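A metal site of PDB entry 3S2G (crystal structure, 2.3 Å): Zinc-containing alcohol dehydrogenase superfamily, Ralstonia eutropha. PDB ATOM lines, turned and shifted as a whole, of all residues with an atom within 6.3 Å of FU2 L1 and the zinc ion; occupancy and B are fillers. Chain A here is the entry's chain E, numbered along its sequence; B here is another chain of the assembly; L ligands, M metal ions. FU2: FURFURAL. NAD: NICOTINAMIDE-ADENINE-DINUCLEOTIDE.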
ATOM      1  N   CYS A  40      -3.526  -0.793 -12.396  1.00  0.00           N
ATOM      2  CA  CYS A  40      -2.438  -0.933 -11.440  1.00  0.00           C
ATOM      3  C   CYS A  40      -1.845  -2.333 -11.469  1.00  0.00           C
ATOM      4  O   CYS A  40      -2.529  -3.299 -11.793  1.00  0.00           O
ATOM      5  CB  CYS A  40      -2.904  -0.604 -10.020  1.00  0.00           C
ATOM      6  SG  CYS A  40      -1.555  -0.684  -8.806  1.00  0.00           S
ATOM      7  N   HIS A  41      -0.567  -2.440 -11.137  1.00  0.00           N
ATOM      8  CA  HIS A  41       0.103  -3.733 -11.106  1.00  0.00           C
ATOM      9  C   HIS A  41      -0.619  -4.651 -10.135  1.00  0.00           C
ATOM     10  O   HIS A  41      -0.528  -5.876 -10.232  1.00  0.00           O
ATOM     11  CB  HIS A  41       1.567  -3.566 -10.695  1.00  0.00           C
ATOM     12  CG  HIS A  41       2.457  -4.648 -11.233  1.00  0.00           C
ATOM     13  ND1 HIS A  41       2.374  -5.959 -10.813  1.00  0.00           N
ATOM     14  CD2 HIS A  41       3.445  -4.614 -12.148  1.00  0.00           C
ATOM     15  CE1 HIS A  41       3.275  -6.686 -11.446  1.00  0.00           C
ATOM     16  NE2 HIS A  41       3.945  -5.885 -12.257  1.00  0.00           N
ATOM     17  N   THR A  42      -1.337  -4.051  -9.181  1.00  0.00           N
ATOM     18  CA  THR A  42      -2.153  -4.799  -8.233  1.00  0.00           C
ATOM     19  C   THR A  42      -3.211  -5.623  -8.962  1.00  0.00           C
ATOM     20  O   THR A  42      -3.516  -6.748  -8.568  1.00  0.00           O
ATOM     21  CB  THR A  42      -2.841  -3.851  -7.244  1.00  0.00           C
ATOM     22  OG1 THR A  42      -1.895  -3.436  -6.246  1.00  0.00           O
ATOM     23  CG2 THR A  42      -4.019  -4.545  -6.573  1.00  0.00           C
ATOM     24  N   ASP A  43      -3.750  -5.056 -10.039  1.00  0.00           N
ATOM     25  CA  ASP A  43      -4.750  -5.753 -10.841  1.00  0.00           C
ATOM     26  C   ASP A  43      -4.196  -7.071 -11.355  1.00  0.00           C
ATOM     27  O   ASP A  43      -4.880  -8.087 -11.354  1.00  0.00           O
ATOM     28  CB  ASP A  43      -5.205  -4.868 -12.016  1.00  0.00           C
ATOM     29  CG  ASP A  43      -5.798  -3.555 -11.561  1.00  0.00           C
ATOM     30  OD1 ASP A  43      -6.330  -3.497 -10.424  1.00  0.00           O
ATOM     31  OD2 ASP A  43      -5.745  -2.573 -12.322  1.00  0.00           O
ATOM     32  N   TRP A  51      -1.481 -13.350  -4.045  1.00  0.00           N
ATOM     33  CA  TRP A  51      -1.605 -12.958  -2.644  1.00  0.00           C
ATOM     34  C   TRP A  51      -2.306 -13.982  -1.761  1.00  0.00           C
ATOM     35  O   TRP A  51      -3.183 -14.729  -2.221  1.00  0.00           O
ATOM     36  CB  TRP A  51      -2.299 -11.600  -2.549  1.00  0.00           C
ATOM     37  CG  TRP A  51      -1.539 -10.514  -3.245  1.00  0.00           C
ATOM     38  CD1 TRP A  51      -0.268 -10.577  -3.731  1.00  0.00           C
ATOM     39  CD2 TRP A  51      -2.010  -9.190  -3.552  1.00  0.00           C
ATOM     40  NE1 TRP A  51       0.091  -9.387  -4.314  1.00  0.00           N
ATOM     41  CE2 TRP A  51      -0.964  -8.514  -4.214  1.00  0.00           C
ATOM     42  CE3 TRP A  51      -3.208  -8.511  -3.320  1.00  0.00           C
ATOM     43  CZ2 TRP A  51      -1.078  -7.195  -4.644  1.00  0.00           C
ATOM     44  CZ3 TRP A  51      -3.322  -7.201  -3.760  1.00  0.00           C
ATOM     45  CH2 TRP A  51      -2.266  -6.559  -4.411  1.00  0.00           C
ATOM     46  N   HIS A  63      -9.289  -0.205  -9.386  1.00  0.00           N
ATOM     47  CA  HIS A  63      -9.449   0.712  -8.262  1.00  0.00           C
ATOM     48  C   HIS A  63      -8.865   2.088  -8.583  1.00  0.00           C
ATOM     49  O   HIS A  63      -8.586   2.881  -7.691  1.00  0.00           O
ATOM     50  CB  HIS A  63      -8.800   0.141  -6.998  1.00  0.00           C
ATOM     51  CG  HIS A  63      -7.422  -0.386  -7.212  1.00  0.00           C
ATOM     52  ND1 HIS A  63      -7.178  -1.635  -7.733  1.00  0.00           N
ATOM     53  CD2 HIS A  63      -6.206   0.167  -6.979  1.00  0.00           C
ATOM     54  CE1 HIS A  63      -5.875  -1.833  -7.809  1.00  0.00           C
ATOM     55  NE2 HIS A  63      -5.261  -0.754  -7.371  1.00  0.00           N
ATOM     56  N   GLU A  64      -8.680   2.351  -9.868  1.00  0.00           N
ATOM     57  CA  GLU A  64      -8.309   3.683 -10.332  1.00  0.00           C
ATOM     58  C   GLU A  64      -9.365   4.193 -11.313  1.00  0.00           C
ATOM     59  O   GLU A  64      -9.057   4.861 -12.297  1.00  0.00           O
ATOM     60  CB  GLU A  64      -6.932   3.670 -11.007  1.00  0.00           C
ATOM     61  CG  GLU A  64      -5.791   3.368 -10.062  1.00  0.00           C
ATOM     62  CD  GLU A  64      -4.440   3.699 -10.656  1.00  0.00           C
ATOM     63  OE1 GLU A  64      -4.297   3.590 -11.894  1.00  0.00           O
ATOM     64  OE2 GLU A  64      -3.537   4.092  -9.893  1.00  0.00           O
ATOM     65  N   TRP A  89      -8.788   1.976  -4.039  1.00  0.00           N
ATOM     66  CA  TRP A  89      -8.619   0.677  -3.383  1.00  0.00           C
ATOM     67  C   TRP A  89      -9.461   0.567  -2.113  1.00  0.00           C
ATOM     68  O   TRP A  89     -10.173  -0.413  -1.913  1.00  0.00           O
ATOM     69  CB  TRP A  89      -7.132   0.454  -3.068  1.00  0.00           C
ATOM     70  CG  TRP A  89      -6.839  -0.838  -2.372  1.00  0.00           C
ATOM     71  CD1 TRP A  89      -6.499  -0.995  -1.057  1.00  0.00           C
ATOM     72  CD2 TRP A  89      -6.867  -2.152  -2.944  1.00  0.00           C
ATOM     73  NE1 TRP A  89      -6.308  -2.334  -0.779  1.00  0.00           N
ATOM     74  CE2 TRP A  89      -6.526  -3.061  -1.920  1.00  0.00           C
ATOM     75  CE3 TRP A  89      -7.137  -2.640  -4.222  1.00  0.00           C
ATOM     76  CZ2 TRP A  89      -6.453  -4.430  -2.143  1.00  0.00           C
ATOM     77  CZ3 TRP A  89      -7.070  -4.015  -4.439  1.00  0.00           C
ATOM     78  CH2 TRP A  89      -6.727  -4.891  -3.397  1.00  0.00           C
ATOM     79  N   ASN A 113     -12.286  -3.705  -0.482  1.00  0.00           N
ATOM     80  CA  ASN A 113     -11.334  -3.197  -1.453  1.00  0.00           C
ATOM     81  C   ASN A 113     -11.855  -3.231  -2.894  1.00  0.00           C
ATOM     82  O   ASN A 113     -12.246  -4.272  -3.406  1.00  0.00           O
ATOM     83  CB  ASN A 113     -10.002  -3.955  -1.346  1.00  0.00           C
ATOM     84  CG  ASN A 113      -9.377  -3.832   0.044  1.00  0.00           C
ATOM     85  OD1 ASN A 113      -9.134  -4.824   0.719  1.00  0.00           O
ATOM     86  ND2 ASN A 113      -9.118  -2.598   0.467  1.00  0.00           N
ATOM     87  N   CYS A 150      -4.548   5.831  -7.054  1.00  0.00           N
ATOM     88  CA  CYS A 150      -3.765   4.825  -6.336  1.00  0.00           C
ATOM     89  C   CYS A 150      -2.261   5.089  -6.373  1.00  0.00           C
ATOM     90  O   CYS A 150      -1.644   5.266  -5.330  1.00  0.00           O
ATOM     91  CB  CYS A 150      -4.065   3.424  -6.863  1.00  0.00           C
ATOM     92  SG  CYS A 150      -3.424   2.141  -5.772  1.00  0.00           S
ATOM     93  N   ALA A 151      -1.690   5.090  -7.567  1.00  0.00           N
ATOM     94  CA  ALA A 151      -0.268   5.365  -7.722  1.00  0.00           C
ATOM     95  C   ALA A 151       0.114   6.655  -7.005  1.00  0.00           C
ATOM     96  O   ALA A 151       1.141   6.718  -6.317  1.00  0.00           O
ATOM     97  CB  ALA A 151       0.104   5.454  -9.191  1.00  0.00           C
ATOM     98  N   THR A 154      -0.658   6.598  -2.966  1.00  0.00           N
ATOM     99  CA  THR A 154       0.210   5.593  -2.371  1.00  0.00           C
ATOM    100  C   THR A 154       1.612   6.112  -2.113  1.00  0.00           C
ATOM    101  O   THR A 154       2.148   5.962  -1.014  1.00  0.00           O
ATOM    102  CB  THR A 154       0.298   4.330  -3.259  1.00  0.00           C
ATOM    103  OG1 THR A 154      -0.935   3.611  -3.195  1.00  0.00           O
ATOM    104  CG2 THR A 154       1.439   3.443  -2.796  1.00  0.00           C
ATOM    105  N   LEU A 178       3.865   3.752  -9.988  1.00  0.00           N
ATOM    106  CA  LEU A 178       4.026   4.472  -8.720  1.00  0.00           C
ATOM    107  C   LEU A 178       5.282   5.321  -8.751  1.00  0.00           C
ATOM    108  O   LEU A 178       5.259   6.492  -8.371  1.00  0.00           O
ATOM    109  CB  LEU A 178       4.124   3.475  -7.556  1.00  0.00           C
ATOM    110  CG  LEU A 178       2.829   3.066  -6.848  1.00  0.00           C
ATOM    111  CD1 LEU A 178       1.871   2.396  -7.822  1.00  0.00           C
ATOM    112  CD2 LEU A 178       3.154   2.151  -5.692  1.00  0.00           C
ATOM    113  N   LEU A 264       4.547  -4.935  -3.533  1.00  0.00           N
ATOM    114  CA  LEU A 264       3.910  -6.122  -2.957  1.00  0.00           C
ATOM    115  C   LEU A 264       4.214  -7.415  -3.703  1.00  0.00           C
ATOM    116  O   LEU A 264       3.305  -8.190  -3.999  1.00  0.00           O
ATOM    117  CB  LEU A 264       2.399  -5.914  -2.882  1.00  0.00           C
ATOM    118  CG  LEU A 264       1.902  -4.957  -1.803  1.00  0.00           C
ATOM    119  CD1 LEU A 264       0.407  -4.724  -1.943  1.00  0.00           C
ATOM    120  CD2 LEU A 264       2.228  -5.507  -0.434  1.00  0.00           C
ATOM    121  N   ILE A 287       0.618   1.445   3.236  1.00  0.00           N
ATOM    122  CA  ILE A 287      -0.503   0.936   2.455  1.00  0.00           C
ATOM    123  C   ILE A 287      -1.399   2.055   1.912  1.00  0.00           C
ATOM    124  O   ILE A 287      -2.055   2.763   2.675  1.00  0.00           O
ATOM    125  CB  ILE A 287      -1.344  -0.053   3.290  1.00  0.00           C
ATOM    126  CG1 ILE A 287      -2.487  -0.623   2.461  1.00  0.00           C
ATOM    127  CG2 ILE A 287      -1.838   0.608   4.572  1.00  0.00           C
ATOM    128  CD1 ILE A 287      -2.026  -1.483   1.325  1.00  0.00           C
ATOM    129  N   VAL A 288      -1.434   2.182   0.588  1.00  0.00           N
ATOM    130  CA  VAL A 288      -2.165   3.256  -0.082  1.00  0.00           C
ATOM    131  C   VAL A 288      -2.170   4.537   0.734  1.00  0.00           C
ATOM    132  O   VAL A 288      -1.127   5.002   1.208  1.00  0.00           O
ATOM    133  CB  VAL A 288      -3.622   2.847  -0.435  1.00  0.00           C
ATOM    134  CG1 VAL A 288      -3.640   1.923  -1.634  1.00  0.00           C
ATOM    135  CG2 VAL A 288      -4.332   2.220   0.768  1.00  0.00           C
ATOM    136  N   ARG A 333       2.129   4.827 -16.422  1.00  0.00           N
ATOM    137  CA  ARG A 333       0.843   4.158 -16.206  1.00  0.00           C
ATOM    138  C   ARG A 333       0.066   3.972 -17.496  1.00  0.00           C
ATOM    139  O   ARG A 333       0.195   4.755 -18.435  1.00  0.00           O
ATOM    140  CB  ARG A 333       0.001   4.977 -15.220  1.00  0.00           C
ATOM    141  CG  ARG A 333       0.055   4.483 -13.783  1.00  0.00           C
ATOM    142  CD  ARG A 333      -0.882   3.312 -13.580  1.00  0.00           C
ATOM    143  NE  ARG A 333      -1.237   3.157 -12.178  1.00  0.00           N
ATOM    144  CZ  ARG A 333      -0.614   2.349 -11.329  1.00  0.00           C
ATOM    145  NH1 ARG A 333      -0.998   2.274 -10.064  1.00  0.00           N
ATOM    146  NH2 ARG A 333       0.391   1.594 -11.753  1.00  0.00           N
ATOM    147  N   PHE B 274       4.371  -8.771   2.098  1.00  0.00           N
ATOM    148  CA  PHE B 274       2.915  -8.596   2.056  1.00  0.00           C
ATOM    149  C   PHE B 274       2.361  -8.178   3.413  1.00  0.00           C
ATOM    150  O   PHE B 274       1.591  -7.224   3.509  1.00  0.00           O
ATOM    151  CB  PHE B 274       2.229  -9.872   1.574  1.00  0.00           C
ATOM    152  CG  PHE B 274       0.759  -9.686   1.291  1.00  0.00           C
ATOM    153  CD1 PHE B 274       0.334  -9.236   0.052  1.00  0.00           C
ATOM    154  CD2 PHE B 274      -0.186  -9.962   2.261  1.00  0.00           C
ATOM    155  CE1 PHE B 274      -1.013  -9.062  -0.211  1.00  0.00           C
ATOM    156  CE2 PHE B 274      -1.533  -9.788   1.998  1.00  0.00           C
ATOM    157  CZ  PHE B 274      -1.952  -9.337   0.766  1.00  0.00           C
ATOM    158  N   LEU B 278       0.809  -4.449   3.947  1.00  0.00           N
ATOM    159  CA  LEU B 278      -0.637  -4.458   4.158  1.00  0.00           C
ATOM    160  C   LEU B 278      -1.021  -4.072   5.578  1.00  0.00           C
ATOM    161  O   LEU B 278      -2.035  -3.404   5.804  1.00  0.00           O
ATOM    162  CB  LEU B 278      -1.225  -5.833   3.826  1.00  0.00           C
ATOM    163  CG  LEU B 278      -1.817  -6.003   2.420  1.00  0.00           C
ATOM    164  CD1 LEU B 278      -3.004  -5.055   2.231  1.00  0.00           C
ATOM    165  CD2 LEU B 278      -0.757  -5.765   1.350  1.00  0.00           C
HETATM  166  C1  FU2 L   1      -3.310  -0.933  -4.073  1.00  0.00           C
HETATM  167  C2  FU2 L   1      -3.191  -1.967  -3.011  1.00  0.00           C
HETATM  168  O3  FU2 L   1      -2.782  -3.238  -3.190  1.00  0.00           O
HETATM  169  C4  FU2 L   1      -2.814  -3.907  -2.027  1.00  0.00           C
HETATM  170  C5  FU2 L   1      -3.273  -3.039  -1.052  1.00  0.00           C
HETATM  171  C6  FU2 L   1      -3.511  -1.811  -1.675  1.00  0.00           C
HETATM  172  OXT FU2 L   1      -3.035  -1.338  -5.359  1.00  0.00           O
HETATM  173  PA  NAD L   2       4.834  -1.027 -12.200  1.00  0.00           P
HETATM  174  O1A NAD L   2       4.080   0.069 -12.869  1.00  0.00           O
HETATM  175  O2A NAD L   2       4.949  -2.224 -13.151  1.00  0.00           O
HETATM  176  O5B NAD L   2       6.285  -0.499 -11.801  1.00  0.00           O
HETATM  177  C5B NAD L   2       7.225  -1.342 -11.351  1.00  0.00           C
HETATM  178  C4B NAD L   2       8.620  -0.871 -11.472  1.00  0.00           C
HETATM  179  O4B NAD L   2       9.487  -1.645 -10.715  1.00  0.00           O
HETATM  180  C3B NAD L   2       9.030  -0.979 -12.879  1.00  0.00           C
HETATM  181  O3B NAD L   2       9.503   0.254 -13.329  1.00  0.00           O
HETATM  182  C2B NAD L   2      10.096  -1.871 -12.904  1.00  0.00           C
HETATM  183  O2B NAD L   2      11.083  -1.390 -13.767  1.00  0.00           O
HETATM  184  C1B NAD L   2      10.603  -1.813 -11.522  1.00  0.00           C
HETATM  185  N9A NAD L   2      11.531  -2.906 -11.025  1.00  0.00           N
HETATM  186  C8A NAD L   2      11.433  -4.233 -11.233  1.00  0.00           C
HETATM  187  N7A NAD L   2      12.474  -4.843 -10.640  1.00  0.00           N
HETATM  188  C5A NAD L   2      13.250  -3.899 -10.045  1.00  0.00           C
HETATM  189  C6A NAD L   2      14.434  -3.899  -9.303  1.00  0.00           C
HETATM  190  N6A NAD L   2      15.087  -5.106  -9.013  1.00  0.00           N
HETATM  191  N1A NAD L   2      14.942  -2.734  -8.847  1.00  0.00           N
HETATM  192  C2A NAD L   2      14.318  -1.576  -9.124  1.00  0.00           C
HETATM  193  N3A NAD L   2      13.183  -1.527  -9.838  1.00  0.00           N
HETATM  194  C4A NAD L   2      12.646  -2.670 -10.301  1.00  0.00           C
HETATM  195  O3  NAD L   2       4.026  -1.473 -10.875  1.00  0.00           O
HETATM  196  PN  NAD L   2       3.218  -0.377 -10.041  1.00  0.00           P
HETATM  197  O1N NAD L   2       3.870   0.997 -10.261  1.00  0.00           O
HETATM  198  O2N NAD L   2       1.725  -0.346 -10.535  1.00  0.00           O
HETATM  199  O5D NAD L   2       3.258  -0.722  -8.518  1.00  0.00           O
HETATM  200  C5D NAD L   2       4.341  -1.373  -7.978  1.00  0.00           C
HETATM  201  C4D NAD L   2       4.081  -2.244  -6.860  1.00  0.00           C
HETATM  202  O4D NAD L   2       3.373  -1.522  -5.807  1.00  0.00           O
HETATM  203  C3D NAD L   2       3.184  -3.344  -7.283  1.00  0.00           C
HETATM  204  O3D NAD L   2       3.604  -4.507  -6.744  1.00  0.00           O
HETATM  205  C2D NAD L   2       1.860  -3.004  -6.759  1.00  0.00           C
HETATM  206  O2D NAD L   2       1.162  -4.140  -6.445  1.00  0.00           O
HETATM  207  C1D NAD L   2       2.229  -2.290  -5.503  1.00  0.00           C
HETATM  208  N1N NAD L   2       1.200  -1.496  -4.806  1.00  0.00           N
HETATM  209  C2N NAD L   2       0.980  -1.251  -3.387  1.00  0.00           C
HETATM  210  C3N NAD L   2       0.635   0.166  -3.002  1.00  0.00           C
HETATM  211  C7N NAD L   2       0.038   0.161  -1.562  1.00  0.00           C
HETATM  212  O7N NAD L   2      -1.228   0.236  -1.385  1.00  0.00           O
HETATM  213  N7N NAD L   2       0.907  -0.079  -0.456  1.00  0.00           N
HETATM  214  C4N NAD L   2      -0.249   0.851  -3.898  1.00  0.00           C
HETATM  215  C5N NAD L   2      -0.370   0.242  -5.222  1.00  0.00           C
HETATM  216  C6N NAD L   2       0.918  -0.364  -5.635  1.00  0.00           C
HETATM  217 ZN    ZN M   1      -3.164   0.050  -7.051  1.00  0.00          ZN
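OG1 of Thr 42 is in hydrogen-bond range of O3 of FU2 L1, 3.2 Å away. The side-chain sulfur (SG) of Cys 40 lies close to an oxygen (O2N) of NAD L2 (3.7 Å). OG1 of Thr 42 is in hydrogen-bond range of O2D of NAD L2 (3.1 Å). The backbone NH (N) of Leu 264 is in hydrogen-bond range of an oxygen (O3D) of NAD L2 (3.4 Å). An oxygen (O7N) of NAD L2 sits at hydrogen-bond distance from the backbone NH of Val 288. NH2 of Arg 333 is in salt-bridge range of O2N of NAD L2, at 2.7 Å. O2N of NAD L2 sits at hydrogen-bond distance from N of His 41 (3.2 Å). The backbone NH (N) of Leu 178 is in hydrogen-bond range of an oxygen (O1N) of NAD L2 (2.8 Å).
ND1 of His 63 lies close to OD1 of Asp 43 (3.4 Å). The side-chain carboxylate (OE2) of Glu 64 sits close to the backbone NH (N) of Cys 150. The backbone carbonyl oxygen (O) of Cys 150 sits at hydrogen-bond distance from the side-chain hydroxyl (OG1) of Thr 154. SG of Cys 40 sits close to N of Thr 42 (3.4 Å). SG of Cys 40 sits close to NH1 of Arg 333, at 3.3 Å. The backbone NH of Cys 40 is in hydrogen-bond range of the side-chain carboxylate of Asp 43, 2.8 Å away. The side-chain amide nitrogen of Asn 113 lies close to the indole nitrogen of Trp 89 (3.1 Å). The indole nitrogen of Trp 51 lies within hydrogen-bond range of the backbone carbonyl oxygen of Leu 264.
Merely in contact with FU2 L1: Trp 89 (3.0 Å), Ile 287 (3.1 Å), Leu 264 (3.3 Å), Trp 51 (3.6 Å), Val 288 (3.7 Å) and Leu 278 of chain B (3.9 Å). Hydrophobic or aromatic side chains within 4 Å of FU2 L1: Trp 51, His 63, Trp 89, Leu 264, Ile 287, Val 288 and Leu 278 of chain B. Within 4 Å of FU2 L1: Cys 40, Thr 42, Trp 51, His 63, Trp 89, Cys 150, Leu 264, Ile 287, Val 288 and Leu 278 of chain B. The nearest printed residue that does not touch FU2 L1 is Thr 154 (5.2 Å).
Thr 42 touches the zinc ion (OG1 to ZN, 3.8 Å). Within 4 Å of the zinc ion: Cys 40, Thr 42, His 63 and Cys 150.
The zinc ion is bound by OXT of FU2 L1 (2.2 Å), NE2 of His 63 (2.3 Å), SG of Cys 150 (2.5 Å) and SG of Cys 40 (2.5 Å).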
